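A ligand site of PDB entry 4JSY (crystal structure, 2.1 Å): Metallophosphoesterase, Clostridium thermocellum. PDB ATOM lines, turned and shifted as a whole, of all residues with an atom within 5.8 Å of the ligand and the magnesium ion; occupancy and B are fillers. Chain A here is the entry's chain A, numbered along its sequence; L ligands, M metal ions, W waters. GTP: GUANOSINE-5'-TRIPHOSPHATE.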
ATOM      1  N   GLY A  16      15.410  15.501 -26.208  1.00  0.00           N
ATOM      2  CA  GLY A  16      15.507  14.660 -25.033  1.00  0.00           C
ATOM      3  C   GLY A  16      16.787  14.814 -24.256  1.00  0.00           C
ATOM      4  O   GLY A  16      17.856  15.121 -24.792  1.00  0.00           O
ATOM      5  N   SER A  17      16.654  14.593 -22.955  1.00  0.00           N
ATOM      6  CA  SER A  17      17.770  14.603 -22.032  1.00  0.00           C
ATOM      7  C   SER A  17      18.910  13.705 -22.481  1.00  0.00           C
ATOM      8  O   SER A  17      18.711  12.776 -23.268  1.00  0.00           O
ATOM      9  CB  SER A  17      17.293  14.122 -20.666  1.00  0.00           C
ATOM     10  OG  SER A  17      18.389  13.969 -19.775  1.00  0.00           O
ATOM     11  N   SER A  18      20.103  13.994 -21.995  1.00  0.00           N
ATOM     12  CA  SER A  18      21.203  13.057 -22.102  1.00  0.00           C
ATOM     13  C   SER A  18      20.745  11.726 -21.508  1.00  0.00           C
ATOM     14  O   SER A  18      20.161  11.695 -20.425  1.00  0.00           O
ATOM     15  CB  SER A  18      22.427  13.579 -21.348  1.00  0.00           C
ATOM     16  OG  SER A  18      23.385  12.551 -21.198  1.00  0.00           O
ATOM     17  N   GLY A  19      20.983  10.640 -22.230  1.00  0.00           N
ATOM     18  CA  GLY A  19      20.580   9.318 -21.760  1.00  0.00           C
ATOM     19  C   GLY A  19      19.167   8.898 -22.134  1.00  0.00           C
ATOM     20  O   GLY A  19      18.744   7.792 -21.796  1.00  0.00           O
ATOM     21  N   SER A  20      18.441   9.759 -22.829  1.00  0.00           N
ATOM     22  CA  SER A  20      17.053   9.443 -23.174  1.00  0.00           C
ATOM     23  C   SER A  20      16.969   8.457 -24.349  1.00  0.00           C
ATOM     24  O   SER A  20      15.915   7.905 -24.610  1.00  0.00           O
ATOM     25  CB  SER A  20      16.227  10.703 -23.462  1.00  0.00           C
ATOM     26  OG  SER A  20      16.725  11.410 -24.591  1.00  0.00           O
ATOM     27  N   GLY A  21      18.100   8.234 -25.015  1.00  0.00           N
ATOM     28  CA  GLY A  21      18.163   7.255 -26.078  1.00  0.00           C
ATOM     29  C   GLY A  21      18.071   7.809 -27.490  1.00  0.00           C
ATOM     30  O   GLY A  21      17.764   7.076 -28.421  1.00  0.00           O
ATOM     31  N   LYS A  22      18.368   9.101 -27.652  1.00  0.00           N
ATOM     32  CA  LYS A  22      18.277   9.744 -28.963  1.00  0.00           C
ATOM     33  C   LYS A  22      19.148   9.078 -30.017  1.00  0.00           C
ATOM     34  O   LYS A  22      18.673   8.731 -31.101  1.00  0.00           O
ATOM     35  CB  LYS A  22      18.615  11.234 -28.862  1.00  0.00           C
ATOM     36  CG  LYS A  22      17.725  12.000 -27.895  1.00  0.00           C
ATOM     37  CD  LYS A  22      18.082  13.481 -27.888  1.00  0.00           C
ATOM     38  CE  LYS A  22      19.541  13.696 -27.463  1.00  0.00           C
ATOM     39  NZ  LYS A  22      19.777  13.263 -26.053  1.00  0.00           N
ATOM     40  N   SER A  23      20.428   8.895 -29.700  1.00  0.00           N
ATOM     41  CA  SER A  23      21.376   8.343 -30.668  1.00  0.00           C
ATOM     42  C   SER A  23      21.049   6.899 -30.994  1.00  0.00           C
ATOM     43  O   SER A  23      21.139   6.477 -32.144  1.00  0.00           O
ATOM     44  CB  SER A  23      22.827   8.442 -30.151  1.00  0.00           C
ATOM     45  OG  SER A  23      23.178   9.790 -29.841  1.00  0.00           O
ATOM     46  N   THR A  24      20.674   6.141 -29.962  1.00  0.00           N
ATOM     47  CA  THR A  24      20.220   4.767 -30.156  1.00  0.00           C
ATOM     48  C   THR A  24      19.023   4.744 -31.103  1.00  0.00           C
ATOM     49  O   THR A  24      18.985   3.971 -32.054  1.00  0.00           O
ATOM     50  CB  THR A  24      19.828   4.118 -28.821  1.00  0.00           C
ATOM     51  OG1 THR A  24      20.930   4.180 -27.903  1.00  0.00           O
ATOM     52  CG2 THR A  24      19.416   2.658 -29.023  1.00  0.00           C
ATOM     53  N   PHE A  25      18.068   5.625 -30.829  1.00  0.00           N
ATOM     54  CA  PHE A  25      16.868   5.751 -31.649  1.00  0.00           C
ATOM     55  C   PHE A  25      17.232   6.100 -33.094  1.00  0.00           C
ATOM     56  O   PHE A  25      16.731   5.479 -34.021  1.00  0.00           O
ATOM     57  CB  PHE A  25      15.965   6.833 -31.045  1.00  0.00           C
ATOM     58  CG  PHE A  25      14.653   7.046 -31.751  1.00  0.00           C
ATOM     59  CD1 PHE A  25      14.551   7.966 -32.799  1.00  0.00           C
ATOM     60  CD2 PHE A  25      13.507   6.385 -31.337  1.00  0.00           C
ATOM     61  CE1 PHE A  25      13.342   8.193 -33.423  1.00  0.00           C
ATOM     62  CE2 PHE A  25      12.288   6.609 -31.961  1.00  0.00           C
ATOM     63  CZ  PHE A  25      12.201   7.510 -33.008  1.00  0.00           C
ATOM     64  N   ASP A  79      20.630  15.119 -34.033  1.00  0.00           N
ATOM     65  CA  ASP A  79      20.779  14.319 -32.829  1.00  0.00           C
ATOM     66  C   ASP A  79      21.570  15.110 -31.803  1.00  0.00           C
ATOM     67  O   ASP A  79      22.794  14.992 -31.704  1.00  0.00           O
ATOM     68  CB  ASP A  79      21.469  12.980 -33.166  1.00  0.00           C
ATOM     69  CG  ASP A  79      21.715  12.127 -31.937  1.00  0.00           C
ATOM     70  OD1 ASP A  79      21.068  12.370 -30.896  1.00  0.00           O
ATOM     71  OD2 ASP A  79      22.566  11.199 -32.005  1.00  0.00           O
ATOM     72  N   ALA A  80      20.846  15.926 -31.047  1.00  0.00           N
ATOM     73  CA  ALA A  80      21.412  16.714 -29.974  1.00  0.00           C
ATOM     74  C   ALA A  80      20.322  16.795 -28.917  1.00  0.00           C
ATOM     75  O   ALA A  80      19.205  16.328 -29.160  1.00  0.00           O
ATOM     76  CB  ALA A  80      21.786  18.101 -30.480  1.00  0.00           C
ATOM     77  N   THR A  81      20.615  17.373 -27.764  1.00  0.00           N
ATOM     78  CA  THR A  81      19.630  17.412 -26.687  1.00  0.00           C
ATOM     79  C   THR A  81      18.408  18.230 -27.093  1.00  0.00           C
ATOM     80  O   THR A  81      17.270  17.785 -26.911  1.00  0.00           O
ATOM     81  CB  THR A  81      20.229  17.952 -25.373  1.00  0.00           C
ATOM     82  OG1 THR A  81      20.543  19.337 -25.524  1.00  0.00           O
ATOM     83  CG2 THR A  81      21.507  17.185 -25.031  1.00  0.00           C
ATOM     84  N   ARG A 117      19.963   4.791 -17.198  1.00  0.00           N
ATOM     85  CA  ARG A 117      20.722   4.455 -18.405  1.00  0.00           C
ATOM     86  C   ARG A 117      22.102   5.108 -18.411  1.00  0.00           C
ATOM     87  O   ARG A 117      23.087   4.525 -18.865  1.00  0.00           O
ATOM     88  CB  ARG A 117      19.945   4.882 -19.651  1.00  0.00           C
ATOM     89  CG  ARG A 117      18.689   4.074 -19.915  1.00  0.00           C
ATOM     90  CD  ARG A 117      17.955   4.619 -21.115  1.00  0.00           C
ATOM     91  NE  ARG A 117      16.837   3.776 -21.517  1.00  0.00           N
ATOM     92  CZ  ARG A 117      15.949   4.117 -22.449  1.00  0.00           C
ATOM     93  NH1 ARG A 117      16.045   5.287 -23.064  1.00  0.00           N
ATOM     94  NH2 ARG A 117      14.966   3.287 -22.743  1.00  0.00           N
ATOM     95  N   ASN A 118      22.162   6.331 -17.898  1.00  0.00           N
ATOM     96  CA  ASN A 118      23.406   7.078 -17.851  1.00  0.00           C
ATOM     97  C   ASN A 118      24.517   6.332 -17.120  1.00  0.00           C
ATOM     98  O   ASN A 118      25.633   6.227 -17.623  1.00  0.00           O
ATOM     99  CB  ASN A 118      23.173   8.452 -17.206  1.00  0.00           C
ATOM    100  CG  ASN A 118      24.456   9.257 -17.073  1.00  0.00           C
ATOM    101  OD1 ASN A 118      25.103   9.574 -18.070  1.00  0.00           O
ATOM    102  ND2 ASN A 118      24.819   9.581 -15.841  1.00  0.00           N
ATOM    103  N   ASN A 120      25.012   3.349 -16.738  1.00  0.00           N
ATOM    104  CA  ASN A 120      25.441   2.133 -17.409  1.00  0.00           C
ATOM    105  C   ASN A 120      26.006   2.350 -18.813  1.00  0.00           C
ATOM    106  O   ASN A 120      26.261   1.393 -19.542  1.00  0.00           O
ATOM    107  CB  ASN A 120      24.298   1.121 -17.436  1.00  0.00           C
ATOM    108  CG  ASN A 120      23.889   0.699 -16.037  1.00  0.00           C
ATOM    109  OD1 ASN A 120      24.660   0.062 -15.338  1.00  0.00           O
ATOM    110  ND2 ASN A 120      22.673   1.055 -15.626  1.00  0.00           N
ATOM    111  N   ARG A 121      26.220   3.614 -19.183  1.00  0.00           N
ATOM    112  CA  ARG A 121      26.836   3.929 -20.474  1.00  0.00           C
ATOM    113  C   ARG A 121      28.322   3.583 -20.505  1.00  0.00           C
ATOM    114  O   ARG A 121      29.041   3.814 -19.529  1.00  0.00           O
ATOM    115  CB  ARG A 121      26.664   5.411 -20.800  1.00  0.00           C
ATOM    116  CG  ARG A 121      25.246   5.814 -21.072  1.00  0.00           C
ATOM    117  CD  ARG A 121      25.173   7.260 -21.494  1.00  0.00           C
ATOM    118  NE  ARG A 121      25.758   7.493 -22.814  1.00  0.00           N
ATOM    119  CZ  ARG A 121      25.574   8.613 -23.509  1.00  0.00           C
ATOM    120  NH1 ARG A 121      24.820   9.585 -23.015  1.00  0.00           N
ATOM    121  NH2 ARG A 121      26.146   8.755 -24.706  1.00  0.00           N
ATOM    122  N   THR A 122      28.768   3.069 -21.642  1.00  0.00           N
ATOM    123  CA  THR A 122      30.159   2.706 -21.831  1.00  0.00           C
ATOM    124  C   THR A 122      30.932   3.799 -22.577  1.00  0.00           C
ATOM    125  O   THR A 122      32.148   3.915 -22.429  1.00  0.00           O
ATOM    126  CB  THR A 122      30.283   1.377 -22.598  1.00  0.00           C
ATOM    127  OG1 THR A 122      29.527   1.453 -23.811  1.00  0.00           O
ATOM    128  CG2 THR A 122      29.753   0.238 -21.760  1.00  0.00           C
ATOM    129  N   ASP A 123      30.221   4.594 -23.361  1.00  0.00           N
ATOM    130  CA  ASP A 123      30.881   5.637 -24.161  1.00  0.00           C
ATOM    131  C   ASP A 123      31.275   6.854 -23.332  1.00  0.00           C
ATOM    132  O   ASP A 123      32.444   7.248 -23.317  1.00  0.00           O
ATOM    133  CB  ASP A 123      30.006   6.048 -25.363  1.00  0.00           C
ATOM    134  CG  ASP A 123      28.558   6.338 -24.974  1.00  0.00           C
ATOM    135  OD1 ASP A 123      28.060   5.769 -23.982  1.00  0.00           O
ATOM    136  OD2 ASP A 123      27.918   7.144 -25.689  1.00  0.00           O
ATOM    137  N   ARG A 124      30.303   7.457 -22.650  1.00  0.00           N
ATOM    138  CA  ARG A 124      30.539   8.609 -21.792  1.00  0.00           C
ATOM    139  C   ARG A 124      29.330   8.805 -20.894  1.00  0.00           C
ATOM    140  O   ARG A 124      28.228   8.351 -21.210  1.00  0.00           O
ATOM    141  CB  ARG A 124      30.780   9.866 -22.628  1.00  0.00           C
ATOM    142  CG  ARG A 124      29.633  10.171 -23.555  1.00  0.00           C
ATOM    143  CD  ARG A 124      29.914  11.340 -24.489  1.00  0.00           C
ATOM    144  NE  ARG A 124      28.955  11.337 -25.591  1.00  0.00           N
ATOM    145  CZ  ARG A 124      27.698  11.767 -25.479  1.00  0.00           C
ATOM    146  NH1 ARG A 124      27.250  12.253 -24.329  1.00  0.00           N
ATOM    147  NH2 ARG A 124      26.890  11.707 -26.527  1.00  0.00           N
ATOM    148  N   VAL A 126      27.316  11.648 -17.947  1.00  0.00           N
ATOM    149  CA  VAL A 126      27.234  12.987 -17.383  1.00  0.00           C
ATOM    150  C   VAL A 126      26.840  12.913 -15.910  1.00  0.00           C
ATOM    151  O   VAL A 126      26.397  11.867 -15.426  1.00  0.00           O
ATOM    152  CB  VAL A 126      26.237  13.883 -18.156  1.00  0.00           C
ATOM    153  CG1 VAL A 126      26.658  14.012 -19.608  1.00  0.00           C
ATOM    154  CG2 VAL A 126      24.825  13.325 -18.066  1.00  0.00           C
ATOM    155  N   PRO A 159       9.533   4.158 -22.537  1.00  0.00           N
ATOM    156  CA  PRO A 159      10.432   3.341 -23.342  1.00  0.00           C
ATOM    157  C   PRO A 159       9.675   2.394 -24.264  1.00  0.00           C
ATOM    158  O   PRO A 159      10.108   2.163 -25.387  1.00  0.00           O
ATOM    159  CB  PRO A 159      11.223   2.556 -22.296  1.00  0.00           C
ATOM    160  CG  PRO A 159      11.232   3.434 -21.109  1.00  0.00           C
ATOM    161  CD  PRO A 159       9.880   4.097 -21.101  1.00  0.00           C
ATOM    162  N   VAL A 162       8.608   4.359 -27.269  1.00  0.00           N
ATOM    163  CA  VAL A 162       9.800   4.594 -28.071  1.00  0.00           C
ATOM    164  C   VAL A 162      10.118   3.347 -28.895  1.00  0.00           C
ATOM    165  O   VAL A 162      10.413   3.441 -30.083  1.00  0.00           O
ATOM    166  CB  VAL A 162      11.018   4.959 -27.193  1.00  0.00           C
ATOM    167  CG1 VAL A 162      12.282   4.996 -28.034  1.00  0.00           C
ATOM    168  CG2 VAL A 162      10.786   6.297 -26.508  1.00  0.00           C
ATOM    169  N   GLU A 163      10.028   2.198 -28.245  1.00  0.00           N
ATOM    170  CA  GLU A 163      10.223   0.892 -28.872  1.00  0.00           C
ATOM    171  C   GLU A 163       9.272   0.613 -30.037  1.00  0.00           C
ATOM    172  O   GLU A 163       9.681   0.058 -31.055  1.00  0.00           O
ATOM    173  CB  GLU A 163      10.044  -0.217 -27.835  1.00  0.00           C
ATOM    174  CG  GLU A 163      11.252  -0.442 -26.942  1.00  0.00           C
ATOM    175  CD  GLU A 163      12.323  -1.268 -27.636  1.00  0.00           C
ATOM    176  OE1 GLU A 163      11.941  -2.098 -28.491  1.00  0.00           O
ATOM    177  OE2 GLU A 163      13.514  -1.078 -27.336  1.00  0.00           O
HETATM  178  PG  GTP L   1      23.319  12.013 -25.250  1.00  0.00           P
HETATM  179  O1G GTP L   1      24.013  11.673 -26.540  1.00  0.00           O
HETATM  180  O2G GTP L   1      24.200  12.052 -24.038  1.00  0.00           O
HETATM  181  O3G GTP L   1      22.384  13.195 -25.363  1.00  0.00           O
HETATM  182  O3B GTP L   1      22.386  10.722 -24.924  1.00  0.00           O
HETATM  183  PB  GTP L   1      21.394   9.980 -25.972  1.00  0.00           P
HETATM  184  O1B GTP L   1      22.043   9.882 -27.333  1.00  0.00           O
HETATM  185  O2B GTP L   1      20.009  10.552 -25.810  1.00  0.00           O
HETATM  186  O3A GTP L   1      21.296   8.504 -25.338  1.00  0.00           O
HETATM  187  PA  GTP L   1      21.966   7.198 -25.998  1.00  0.00           P
HETATM  188  O1A GTP L   1      23.464   7.401 -26.012  1.00  0.00           O
HETATM  189  O2A GTP L   1      21.269   6.841 -27.290  1.00  0.00           O
HETATM  190  O5' GTP L   1      21.591   6.098 -24.884  1.00  0.00           O
HETATM  191  C5' GTP L   1      22.158   6.126 -23.573  1.00  0.00           C
HETATM  192  C4' GTP L   1      22.175   4.722 -22.975  1.00  0.00           C
HETATM  193  O4' GTP L   1      20.852   4.177 -22.884  1.00  0.00           O
HETATM  194  C3' GTP L   1      22.965   3.792 -23.869  1.00  0.00           C
HETATM  195  O3' GTP L   1      23.732   2.915 -23.027  1.00  0.00           O
HETATM  196  C2' GTP L   1      21.933   2.973 -24.601  1.00  0.00           C
HETATM  197  O2' GTP L   1      22.440   1.670 -24.884  1.00  0.00           O
HETATM  198  C1' GTP L   1      20.763   2.953 -23.624  1.00  0.00           C
HETATM  199  N9  GTP L   1      19.487   2.866 -24.366  1.00  0.00           N
HETATM  200  C8  GTP L   1      19.082   3.731 -25.314  1.00  0.00           C
HETATM  201  N7  GTP L   1      17.876   3.368 -25.820  1.00  0.00           N
HETATM  202  C5  GTP L   1      17.488   2.250 -25.193  1.00  0.00           C
HETATM  203  C6  GTP L   1      16.305   1.348 -25.256  1.00  0.00           C
HETATM  204  O6  GTP L   1      15.367   1.584 -26.050  1.00  0.00           O
HETATM  205  N1  GTP L   1      16.281   0.287 -24.431  1.00  0.00           N
HETATM  206  C2  GTP L   1      17.291   0.023 -23.571  1.00  0.00           C
HETATM  207  N2  GTP L   1      17.200  -1.061 -22.775  1.00  0.00           N
HETATM  208  N3  GTP L   1      18.402   0.810 -23.468  1.00  0.00           N
HETATM  209  C4  GTP L   1      18.551   1.915 -24.235  1.00  0.00           C
HETATM  210 MG    MG M   1      23.710  10.787 -28.202  1.00  0.00          MG
HETATM  211  O   HOH W   1      24.836   9.132 -27.608  1.00  0.00           O
HETATM  212  O   HOH W   2      23.101  14.727 -27.359  1.00  0.00           O
HETATM  213  O   HOH W   3      13.689  -0.525 -23.315  1.00  0.00           O
HETATM  214  O   HOH W   4      22.730  12.465 -28.851  1.00  0.00           O
HETATM  215  O   HOH W   5      22.916   2.575 -20.270  1.00  0.00           O
HETATM  216  O   HOH W   6      25.413  11.585 -29.093  1.00  0.00           O
HETATM  217  O   HOH W   7      16.159   4.887 -27.741  1.00  0.00           O
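The magnesium ion is bound by an oxygen (O1G) of the ligand, the side-chain hydroxyl of Ser 23, water W4, water W6, an oxygen (O1B) of the ligand and water W1.
The magnesium ion has six donor atoms within binding distance.
O2A of the ligand lies within hydrogen-bond range of N of Ser 23 (3.3 Å).
O2B of the ligand is in hydrogen-bond range of N of Lys 22 (2.9 Å).
The side-chain amino group (NZ) of Lys 22 is in salt-bridge range of an oxygen (O3G) of the ligand (2.7 Å).
An oxygen (O2G) of the ligand lies within salt-bridge range of the guanidinium group (NH1) of Arg 121 (2.7 Å).
N of Thr 24 is in hydrogen-bond range of O2A of the ligand (2.8 Å).
O2A of the ligand lies within hydrogen-bond range of OG1 of Thr 24.
An oxygen (O2G) of the ligand lies within salt-bridge range of the guanidinium group of Arg 124 (3.1 Å).
The side-chain hydroxyl (OG) of Ser 18 sits at hydrogen-bond distance from an oxygen (O2G) of the ligand, 3.0 Å away.
N of Gly 19 sits at hydrogen-bond distance from O3B of the ligand, at 3.0 Å.
N of Gly 21 lies within hydrogen-bond range of O2B of the ligand (3.1 Å).
O2B of the ligand is in hydrogen-bond range of N of Ser 20 (3.5 Å).
Residues that only touch the magnesium ion: Arg 124 (3.7 Å) and Asp 79 (3.99 Å).
Within 4 Å of the magnesium ion: Ser 23, Asp 79 and Arg 124.
The nearest printed residue that does not touch the magnesium ion is Arg 121 (4.7 Å).
The side-chain carboxylate (OE2) of Glu 163 lies close to an oxygen (O6) of the ligand (3.5 Å).
Ser 17 touches the ligand.
Arg 117 touches the ligand (CD to O4', 3.4 Å).
The nearest printed residue that does not touch the ligand is Thr 81 (4.1 Å).
The side-chain hydroxyl (OG) of Ser 23 sits close to the side-chain carboxylate (OD2) of Asp 79.
NZ of Lys 22 lies within hydrogen-bond range of O of Ser 17 (3.0 Å).
O of Gly 16 is in hydrogen-bond range of NZ of Lys 22 (3.0 Å).
The backbone carbonyl oxygen of Arg 124 lies within hydrogen-bond range of the guanidinium group of Arg 121 (3.1 Å).
The side-chain carboxylate (OD2) of Asp 123 is in salt-bridge range of the guanidinium group (NH2) of Arg 121, at 2.6 Å.
The guanidinium group (NH1) of Arg 117 lies within hydrogen-bond range of the backbone carbonyl oxygen (O) of Ser 20 (3.0 Å).
The backbone carbonyl oxygen (O) of Ser 17 lies within hydrogen-bond range of the side-chain hydroxyl (OG) of Ser 20, 2.7 Å away.
Water W1 lies within hydrogen-bond range of an oxygen (O1A) of the ligand (2.7 Å), the guanidinium group (NH2) of Arg 121 (3.2 Å) and the guanidinium group (NH2) of Arg 124 (3.5 Å).
Water W5 lies within hydrogen-bond range of O of Arg 117 (2.4 Å) and O3' of the ligand (2.9 Å).
Water W7 bridges the backbone carbonyl oxygen of Gly 21 (2.8 Å) and a nitrogen (N7) of the ligand (3.0 Å).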
